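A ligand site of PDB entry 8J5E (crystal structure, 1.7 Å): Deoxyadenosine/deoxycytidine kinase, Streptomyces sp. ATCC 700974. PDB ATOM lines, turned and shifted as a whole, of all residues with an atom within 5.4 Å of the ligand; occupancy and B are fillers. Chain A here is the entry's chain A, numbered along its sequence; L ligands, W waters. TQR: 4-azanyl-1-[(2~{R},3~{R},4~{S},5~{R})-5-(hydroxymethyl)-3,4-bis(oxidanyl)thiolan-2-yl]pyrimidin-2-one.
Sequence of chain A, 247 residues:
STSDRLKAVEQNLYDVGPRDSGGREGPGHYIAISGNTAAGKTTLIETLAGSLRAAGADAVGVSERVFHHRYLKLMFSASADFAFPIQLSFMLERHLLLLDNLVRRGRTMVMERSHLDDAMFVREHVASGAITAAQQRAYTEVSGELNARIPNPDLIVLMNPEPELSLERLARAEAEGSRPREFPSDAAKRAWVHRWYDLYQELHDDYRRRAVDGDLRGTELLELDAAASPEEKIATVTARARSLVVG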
ATOM      1  N   ASN A  36     -12.927   7.976 -32.516  1.00  0.00           N
ATOM      2  CA  ASN A  36     -13.277   8.981 -31.512  1.00  0.00           C
ATOM      3  C   ASN A  36     -14.122   8.343 -30.414  1.00  0.00           C
ATOM      4  O   ASN A  36     -15.316   8.620 -30.254  1.00  0.00           O
ATOM      5  CB  ASN A  36     -14.000  10.145 -32.151  1.00  0.00           C
ATOM      6  CG  ASN A  36     -14.206  11.288 -31.187  1.00  0.00           C
ATOM      7  OD1 ASN A  36     -13.433  11.467 -30.253  1.00  0.00           O
ATOM      8  ND2 ASN A  36     -15.261  12.051 -31.399  1.00  0.00           N
ATOM      9  N   THR A  37     -13.470   7.488 -29.631  1.00  0.00           N
ATOM     10  CA  THR A  37     -14.113   6.763 -28.533  1.00  0.00           C
ATOM     11  C   THR A  37     -14.156   7.631 -27.266  1.00  0.00           C
ATOM     12  O   THR A  37     -13.647   7.270 -26.201  1.00  0.00           O
ATOM     13  CB  THR A  37     -13.374   5.454 -28.306  1.00  0.00           C
ATOM     14  OG1 THR A  37     -11.988   5.714 -28.105  1.00  0.00           O
ATOM     15  CG2 THR A  37     -13.526   4.541 -29.538  1.00  0.00           C
ATOM     16  N   ALA A  38     -14.801   8.799 -27.381  1.00  0.00           N
ATOM     17  CA  ALA A  38     -14.775   9.787 -26.305  1.00  0.00           C
ATOM     18  C   ALA A  38     -15.472   9.284 -25.049  1.00  0.00           C
ATOM     19  O   ALA A  38     -15.177   9.766 -23.945  1.00  0.00           O
ATOM     20  CB  ALA A  38     -15.415  11.099 -26.769  1.00  0.00           C
ATOM     21  N   GLU A  64      -8.262   4.329 -22.069  1.00  0.00           N
ATOM     22  CA  GLU A  64      -7.611   5.621 -21.881  1.00  0.00           C
ATOM     23  C   GLU A  64      -7.662   6.072 -20.435  1.00  0.00           C
ATOM     24  O   GLU A  64      -6.804   6.854 -19.998  1.00  0.00           O
ATOM     25  CB  GLU A  64      -8.233   6.686 -22.789  1.00  0.00           C
ATOM     26  CG  GLU A  64      -8.015   6.481 -24.264  1.00  0.00           C
ATOM     27  CD  GLU A  64      -6.558   6.643 -24.665  1.00  0.00           C
ATOM     28  OE1 GLU A  64      -5.761   5.735 -24.358  1.00  0.00           O
ATOM     29  OE2 GLU A  64      -6.226   7.661 -25.308  1.00  0.00           O
ATOM     30  N   ARG A  65      -8.659   5.622 -19.670  1.00  0.00           N
ATOM     31  CA  ARG A  65      -8.755   6.036 -18.274  1.00  0.00           C
ATOM     32  C   ARG A  65      -7.582   5.552 -17.435  1.00  0.00           C
ATOM     33  O   ARG A  65      -7.463   5.970 -16.281  1.00  0.00           O
ATOM     34  CB  ARG A  65     -10.085   5.562 -17.681  1.00  0.00           C
ATOM     35  CG  ARG A  65     -11.301   5.890 -18.543  1.00  0.00           C
ATOM     36  CD  ARG A  65     -11.401   7.373 -18.895  1.00  0.00           C
ATOM     37  NE  ARG A  65     -11.752   8.197 -17.744  1.00  0.00           N
ATOM     38  CZ  ARG A  65     -11.894   9.520 -17.780  1.00  0.00           C
ATOM     39  NH1 ARG A  65     -11.728  10.206 -18.902  1.00  0.00           N
ATOM     40  NH2 ARG A  65     -12.182  10.177 -16.657  1.00  0.00           N
ATOM     41  N   LEU A  72      -6.362  16.284 -15.865  1.00  0.00           N
ATOM     42  CA  LEU A  72      -7.026  16.199 -17.176  1.00  0.00           C
ATOM     43  C   LEU A  72      -8.009  17.350 -17.424  1.00  0.00           C
ATOM     44  O   LEU A  72      -8.012  17.954 -18.502  1.00  0.00           O
ATOM     45  CB  LEU A  72      -7.752  14.862 -17.319  1.00  0.00           C
ATOM     46  CG  LEU A  72      -8.546  14.737 -18.630  1.00  0.00           C
ATOM     47  CD1 LEU A  72      -7.599  14.809 -19.800  1.00  0.00           C
ATOM     48  CD2 LEU A  72      -9.352  13.444 -18.693  1.00  0.00           C
ATOM     49  N   MET A  75      -7.003  20.589 -19.137  1.00  0.00           N
ATOM     50  CA  MET A  75      -6.636  20.736 -20.541  1.00  0.00           C
ATOM     51  C   MET A  75      -7.812  21.340 -21.301  1.00  0.00           C
ATOM     52  O   MET A  75      -7.618  21.943 -22.373  1.00  0.00           O
ATOM     53  CB  MET A  75      -6.202  19.384 -21.151  1.00  0.00           C
ATOM     54  CG  MET A  75      -6.289  19.311 -22.653  1.00  0.00           C
ATOM     55  SD  MET A  75      -5.177  17.959 -23.213  1.00  0.00           S
ATOM     56  CE  MET A  75      -6.057  16.526 -22.562  1.00  0.00           C
ATOM     57  N   PHE A  76      -9.024  21.218 -20.748  1.00  0.00           N
ATOM     58  CA  PHE A  76     -10.226  21.752 -21.354  1.00  0.00           C
ATOM     59  C   PHE A  76     -10.726  23.026 -20.686  1.00  0.00           C
ATOM     60  O   PHE A  76     -11.406  23.823 -21.350  1.00  0.00           O
ATOM     61  CB  PHE A  76     -11.338  20.696 -21.347  1.00  0.00           C
ATOM     62  CG  PHE A  76     -10.913  19.396 -21.958  1.00  0.00           C
ATOM     63  CD1 PHE A  76     -10.532  19.345 -23.282  1.00  0.00           C
ATOM     64  CD2 PHE A  76     -10.857  18.227 -21.193  1.00  0.00           C
ATOM     65  CE1 PHE A  76     -10.108  18.161 -23.868  1.00  0.00           C
ATOM     66  CE2 PHE A  76     -10.434  17.030 -21.774  1.00  0.00           C
ATOM     67  CZ  PHE A  76     -10.050  17.005 -23.108  1.00  0.00           C
ATOM     68  N   GLN A  87      -0.948  16.898 -23.123  1.00  0.00           N
ATOM     69  CA  GLN A  87      -0.731  16.064 -24.312  1.00  0.00           C
ATOM     70  C   GLN A  87       0.605  15.333 -24.233  1.00  0.00           C
ATOM     71  O   GLN A  87       0.709  14.167 -24.644  1.00  0.00           O
ATOM     72  CB  GLN A  87      -0.820  16.907 -25.585  1.00  0.00           C
ATOM     73  CG  GLN A  87      -2.279  17.250 -26.017  1.00  0.00           C
ATOM     74  CD  GLN A  87      -3.171  16.021 -26.217  1.00  0.00           C
ATOM     75  OE1 GLN A  87      -4.364  16.029 -25.840  1.00  0.00           O
ATOM     76  NE2 GLN A  87      -2.604  14.987 -26.811  1.00  0.00           N
ATOM     77  N   PHE A  90      -0.059  12.224 -22.097  1.00  0.00           N
ATOM     78  CA  PHE A  90      -0.712  11.103 -22.767  1.00  0.00           C
ATOM     79  C   PHE A  90       0.299  10.303 -23.576  1.00  0.00           C
ATOM     80  O   PHE A  90       0.362   9.067 -23.488  1.00  0.00           O
ATOM     81  CB  PHE A  90      -1.826  11.590 -23.685  1.00  0.00           C
ATOM     82  CG  PHE A  90      -3.201  11.618 -23.032  1.00  0.00           C
ATOM     83  CD1 PHE A  90      -3.887  10.448 -22.792  1.00  0.00           C
ATOM     84  CD2 PHE A  90      -3.786  12.825 -22.693  1.00  0.00           C
ATOM     85  CE1 PHE A  90      -5.140  10.465 -22.199  1.00  0.00           C
ATOM     86  CE2 PHE A  90      -5.051  12.850 -22.103  1.00  0.00           C
ATOM     87  CZ  PHE A  90      -5.725  11.672 -21.860  1.00  0.00           C
ATOM     88  N   ARG A  94       1.588   6.496 -22.329  1.00  0.00           N
ATOM     89  CA  ARG A  94       1.302   5.416 -23.268  1.00  0.00           C
ATOM     90  C   ARG A  94       2.597   4.782 -23.737  1.00  0.00           C
ATOM     91  O   ARG A  94       2.707   3.543 -23.831  1.00  0.00           O
ATOM     92  CB  ARG A  94       0.492   5.942 -24.457  1.00  0.00           C
ATOM     93  CG  ARG A  94      -0.185   4.826 -25.283  1.00  0.00           C
ATOM     94  CD  ARG A  94      -0.716   5.338 -26.644  1.00  0.00           C
ATOM     95  NE  ARG A  94      -1.532   6.548 -26.503  1.00  0.00           N
ATOM     96  CZ  ARG A  94      -2.747   6.586 -25.966  1.00  0.00           C
ATOM     97  NH1 ARG A  94      -3.367   5.492 -25.562  1.00  0.00           N
ATOM     98  NH2 ARG A  94      -3.348   7.769 -25.822  1.00  0.00           N
ATOM     99  N   GLU A 112      -7.218   0.876 -26.320  1.00  0.00           N
ATOM    100  CA  GLU A 112      -8.265   1.763 -26.811  1.00  0.00           C
ATOM    101  C   GLU A 112      -7.722   2.731 -27.848  1.00  0.00           C
ATOM    102  O   GLU A 112      -8.448   3.156 -28.751  1.00  0.00           O
ATOM    103  CB  GLU A 112      -8.910   2.547 -25.659  1.00  0.00           C
ATOM    104  CG  GLU A 112     -10.182   3.312 -26.087  1.00  0.00           C
ATOM    105  CD  GLU A 112     -10.658   4.312 -25.047  1.00  0.00           C
ATOM    106  OE1 GLU A 112     -10.498   3.990 -23.840  1.00  0.00           O
ATOM    107  OE2 GLU A 112     -11.232   5.363 -25.419  1.00  0.00           O
ATOM    108  N   ARG A 113      -6.459   3.108 -27.711  1.00  0.00           N
ATOM    109  CA  ARG A 113      -5.807   4.045 -28.617  1.00  0.00           C
ATOM    110  C   ARG A 113      -4.324   3.732 -28.719  1.00  0.00           C
ATOM    111  O   ARG A 113      -3.666   3.513 -27.703  1.00  0.00           O
ATOM    112  CB  ARG A 113      -6.011   5.479 -28.117  1.00  0.00           C
ATOM    113  CG  ARG A 113      -5.470   6.545 -29.073  1.00  0.00           C
ATOM    114  CD  ARG A 113      -5.968   7.925 -28.673  1.00  0.00           C
ATOM    115  NE  ARG A 113      -7.299   8.134 -29.230  1.00  0.00           N
ATOM    116  CZ  ARG A 113      -8.408   8.250 -28.516  1.00  0.00           C
ATOM    117  NH1 ARG A 113      -8.369   8.324 -27.188  1.00  0.00           N
ATOM    118  NH2 ARG A 113      -9.585   8.284 -29.139  1.00  0.00           N
ATOM    119  N   ASP A 118      -2.011   9.932 -30.970  1.00  0.00           N
ATOM    120  CA  ASP A 118      -1.941  11.074 -30.041  1.00  0.00           C
ATOM    121  C   ASP A 118      -1.664  12.387 -30.763  1.00  0.00           C
ATOM    122  O   ASP A 118      -2.144  13.438 -30.327  1.00  0.00           O
ATOM    123  CB  ASP A 118      -0.860  10.845 -28.985  1.00  0.00           C
ATOM    124  CG  ASP A 118      -1.247   9.807 -27.954  1.00  0.00           C
ATOM    125  OD1 ASP A 118      -2.351   9.937 -27.387  1.00  0.00           O
ATOM    126  OD2 ASP A 118      -0.411   8.879 -27.713  1.00  0.00           O
ATOM    127  N   PHE A 121      -4.490  14.797 -31.533  1.00  0.00           N
ATOM    128  CA  PHE A 121      -5.055  15.605 -30.461  1.00  0.00           C
ATOM    129  C   PHE A 121      -4.234  16.855 -30.203  1.00  0.00           C
ATOM    130  O   PHE A 121      -4.779  17.864 -29.753  1.00  0.00           O
ATOM    131  CB  PHE A 121      -5.188  14.752 -29.191  1.00  0.00           C
ATOM    132  CG  PHE A 121      -6.257  13.690 -29.291  1.00  0.00           C
ATOM    133  CD1 PHE A 121      -5.992  12.457 -29.887  1.00  0.00           C
ATOM    134  CD2 PHE A 121      -7.529  13.926 -28.810  1.00  0.00           C
ATOM    135  CE1 PHE A 121      -6.980  11.488 -30.001  1.00  0.00           C
ATOM    136  CE2 PHE A 121      -8.522  12.952 -28.916  1.00  0.00           C
ATOM    137  CZ  PHE A 121      -8.247  11.733 -29.511  1.00  0.00           C
ATOM    138  N   HIS A 125      -5.507  21.044 -30.711  1.00  0.00           N
ATOM    139  CA  HIS A 125      -5.201  22.178 -29.847  1.00  0.00           C
ATOM    140  C   HIS A 125      -4.393  23.238 -30.584  1.00  0.00           C
ATOM    141  O   HIS A 125      -4.445  24.415 -30.213  1.00  0.00           O
ATOM    142  CB  HIS A 125      -4.430  21.702 -28.616  1.00  0.00           C
ATOM    143  CG  HIS A 125      -5.284  21.007 -27.595  1.00  0.00           C
ATOM    144  ND1 HIS A 125      -6.264  21.656 -26.877  1.00  0.00           N
ATOM    145  CD2 HIS A 125      -5.288  19.727 -27.167  1.00  0.00           C
ATOM    146  CE1 HIS A 125      -6.840  20.806 -26.044  1.00  0.00           C
ATOM    147  NE2 HIS A 125      -6.266  19.628 -26.204  1.00  0.00           N
ATOM    148  N   ARG A 179     -18.675   8.932 -14.791  1.00  0.00           N
ATOM    149  CA  ARG A 179     -17.459   9.664 -15.101  1.00  0.00           C
ATOM    150  C   ARG A 179     -17.654  11.140 -14.795  1.00  0.00           C
ATOM    151  O   ARG A 179     -18.788  11.643 -14.888  1.00  0.00           O
ATOM    152  CB  ARG A 179     -17.018   9.404 -16.544  1.00  0.00           C
ATOM    153  CG  ARG A 179     -17.501  10.338 -17.609  1.00  0.00           C
ATOM    154  CD  ARG A 179     -16.412  10.403 -18.680  1.00  0.00           C
ATOM    155  NE  ARG A 179     -16.073   9.092 -19.222  1.00  0.00           N
ATOM    156  CZ  ARG A 179     -15.339   8.896 -20.311  1.00  0.00           C
ATOM    157  NH1 ARG A 179     -14.821   9.909 -20.984  1.00  0.00           N
ATOM    158  NH2 ARG A 179     -15.113   7.648 -20.731  1.00  0.00           N
ATOM    159  N   GLU A 182     -15.757  16.472 -17.500  1.00  0.00           N
ATOM    160  CA  GLU A 182     -14.390  16.921 -17.677  1.00  0.00           C
ATOM    161  C   GLU A 182     -14.287  18.174 -18.542  1.00  0.00           C
ATOM    162  O   GLU A 182     -13.184  18.714 -18.704  1.00  0.00           O
ATOM    163  CB  GLU A 182     -13.538  15.786 -18.226  1.00  0.00           C
ATOM    164  CG  GLU A 182     -12.977  14.994 -17.045  1.00  0.00           C
ATOM    165  CD  GLU A 182     -12.644  13.560 -17.344  1.00  0.00           C
ATOM    166  OE1 GLU A 182     -12.942  13.081 -18.462  1.00  0.00           O
ATOM    167  OE2 GLU A 182     -12.086  12.918 -16.434  1.00  0.00           O
ATOM    168  N   PHE A 183     -15.406  18.677 -19.048  1.00  0.00           N
ATOM    169  CA  PHE A 183     -15.403  19.869 -19.881  1.00  0.00           C
ATOM    170  C   PHE A 183     -16.009  21.053 -19.134  1.00  0.00           C
ATOM    171  O   PHE A 183     -16.799  20.871 -18.202  1.00  0.00           O
ATOM    172  CB  PHE A 183     -16.176  19.593 -21.185  1.00  0.00           C
ATOM    173  CG  PHE A 183     -15.544  18.528 -22.031  1.00  0.00           C
ATOM    174  CD1 PHE A 183     -14.480  18.825 -22.868  1.00  0.00           C
ATOM    175  CD2 PHE A 183     -15.998  17.203 -21.968  1.00  0.00           C
ATOM    176  CE1 PHE A 183     -13.879  17.837 -23.638  1.00  0.00           C
ATOM    177  CE2 PHE A 183     -15.409  16.222 -22.741  1.00  0.00           C
ATOM    178  CZ  PHE A 183     -14.344  16.538 -23.567  1.00  0.00           C
ATOM    179  N   TRP A 196     -12.832  16.294 -32.729  1.00  0.00           N
ATOM    180  CA  TRP A 196     -12.121  15.021 -32.763  1.00  0.00           C
ATOM    181  C   TRP A 196     -12.698  14.084 -33.819  1.00  0.00           C
ATOM    182  O   TRP A 196     -11.954  13.376 -34.510  1.00  0.00           O
ATOM    183  CB  TRP A 196     -12.184  14.356 -31.394  1.00  0.00           C
ATOM    184  CG  TRP A 196     -11.406  15.035 -30.329  1.00  0.00           C
ATOM    185  CD1 TRP A 196     -10.287  15.803 -30.483  1.00  0.00           C
ATOM    186  CD2 TRP A 196     -11.704  15.030 -28.932  1.00  0.00           C
ATOM    187  NE1 TRP A 196      -9.857  16.266 -29.251  1.00  0.00           N
ATOM    188  CE2 TRP A 196     -10.719  15.799 -28.290  1.00  0.00           C
ATOM    189  CE3 TRP A 196     -12.717  14.439 -28.164  1.00  0.00           C
ATOM    190  CZ2 TRP A 196     -10.696  15.982 -26.898  1.00  0.00           C
ATOM    191  CZ3 TRP A 196     -12.710  14.618 -26.784  1.00  0.00           C
ATOM    192  CH2 TRP A 196     -11.699  15.393 -26.161  1.00  0.00           C
HETATM  193  N1  TQR L   1      -7.763  12.315 -25.090  1.00  0.00           N
HETATM  194  N3  TQR L   1      -3.901  12.276 -26.704  1.00  0.00           N
HETATM  195  C4  TQR L   1      -9.117  12.446 -24.523  1.00  0.00           C
HETATM  196  C5  TQR L   1     -10.489   9.745 -22.526  1.00  0.00           C
HETATM  197  C6  TQR L   1      -7.089  13.425 -25.332  1.00  0.00           C
HETATM  198  C7  TQR L   1      -5.242  12.229 -26.164  1.00  0.00           C
HETATM  199  C8  TQR L   1      -5.973  10.921 -25.899  1.00  0.00           C
HETATM  200  C1  TQR L   1     -10.644  11.254 -22.741  1.00  0.00           C
HETATM  201  C2  TQR L   1     -11.302  11.496 -24.086  1.00  0.00           C
HETATM  202  C3  TQR L   1     -10.166  11.502 -25.122  1.00  0.00           C
HETATM  203  C9  TQR L   1      -7.246  11.126 -25.357  1.00  0.00           C
HETATM  204  N2  TQR L   1      -5.799  13.498 -25.877  1.00  0.00           N
HETATM  205  O1  TQR L   1     -11.899  12.760 -24.051  1.00  0.00           O
HETATM  206  O2  TQR L   1     -10.670  12.006 -26.312  1.00  0.00           O
HETATM  207  O3  TQR L   1     -11.405   9.332 -21.556  1.00  0.00           O
HETATM  208  O4  TQR L   1      -7.650  14.642 -25.064  1.00  0.00           O
HETATM  209  S1  TQR L   1      -9.019  12.029 -22.766  1.00  0.00           S
HETATM  210  O   HOH W   1     -12.932   7.802 -23.054  1.00  0.00           O
HETATM  211  O   HOH W   2     -14.476  12.487 -23.413  1.00  0.00           O
HETATM  212  O   HOH W   3     -10.852   8.208 -25.810  1.00  0.00           O
HETATM  213  O   HOH W   4      -7.366  17.102 -25.932  1.00  0.00           O
HETATM  214  O   HOH W   5     -11.832  10.369 -28.111  1.00  0.00           O
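The side-chain carboxylate of Asp 118 sits at hydrogen-bond distance from a nitrogen (N3) of the ligand (2.9 Å). The side-chain amide oxygen (OE1) of Gln 87 lies close to a nitrogen (N2) of the ligand (2.9 Å). O3 of the ligand lies within hydrogen-bond range of NH1 of Arg 65 (2.8 Å).
The side-chain carboxylate (OE2) of Glu 182 is in salt-bridge range of the guanidinium group (NH2) of Arg 65, 2.8 Å away. OE2 of Glu 64 lies within salt-bridge range of NH1 of Arg 113, 2.9 Å away. The backbone NH of Glu 64 lies within hydrogen-bond range of the side-chain carboxylate of Glu 112, 2.9 Å away. OD1 of Asp 118 lies within salt-bridge range of NH2 of Arg 94, at 2.9 Å. The side-chain carboxylate (OE1) of Glu 64 is in salt-bridge range of the guanidinium group (NH1) of Arg 94 (2.7 Å). The backbone carbonyl oxygen (O) of Arg 113 sits at hydrogen-bond distance from the guanidinium group (NH1) of Arg 94, at 2.9 Å. NH1 of Arg 179 sits at hydrogen-bond distance from O of Ala 38, at 3.0 Å. NE2 of His 125 lies close to SD of Met 75, 3.6 Å away.
Glu 64 touches the ligand (OE2 to C8, 3.3 Å). Met 75 touches the ligand. Phe 76 touches the ligand (CZ to O4, 3.9 Å). Phe 90 touches the ligand (CZ to S1, 3.4 Å). Arg 113 touches the ligand (NH1 to C9, 3.5 Å). CD2 of Phe 121 touches N2 of the ligand (3.4 Å). Arg 179 touches the ligand (NH1 to O3, 3.5 Å). Trp 196 touches the ligand. Hydrophobic or aromatic side chains within 4 Å of the ligand: Met 75, Phe 76, Phe 90, Phe 121 and Trp 196. The nearest printed residue that does not touch the ligand is Arg 94 (4.1 Å).
Water W1 lies within hydrogen-bond range of O3 of the ligand (2.6 Å), O of Ala 38 (3.1 Å), NH2 of Arg 179 (3.2 Å) and O of Thr 37 (3.3 Å). Water W2 bridges an oxygen (O1) of the ligand (2.7 Å) and the backbone carbonyl oxygen (O) of Ala 38 (2.9 Å). Water W5 lies within hydrogen-bond range of O2 of the ligand (2.7 Å), OD1 of Asn 36 (2.9 Å), NH2 of Arg 113 (3.2 Å) and N of Ala 38 (3.4 Å). Water W3 lies within hydrogen-bond range of NH1 of Arg 113 (2.8 Å), OE2 of Glu 112 (2.9 Å) and O of Thr 37 (3.0 Å).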
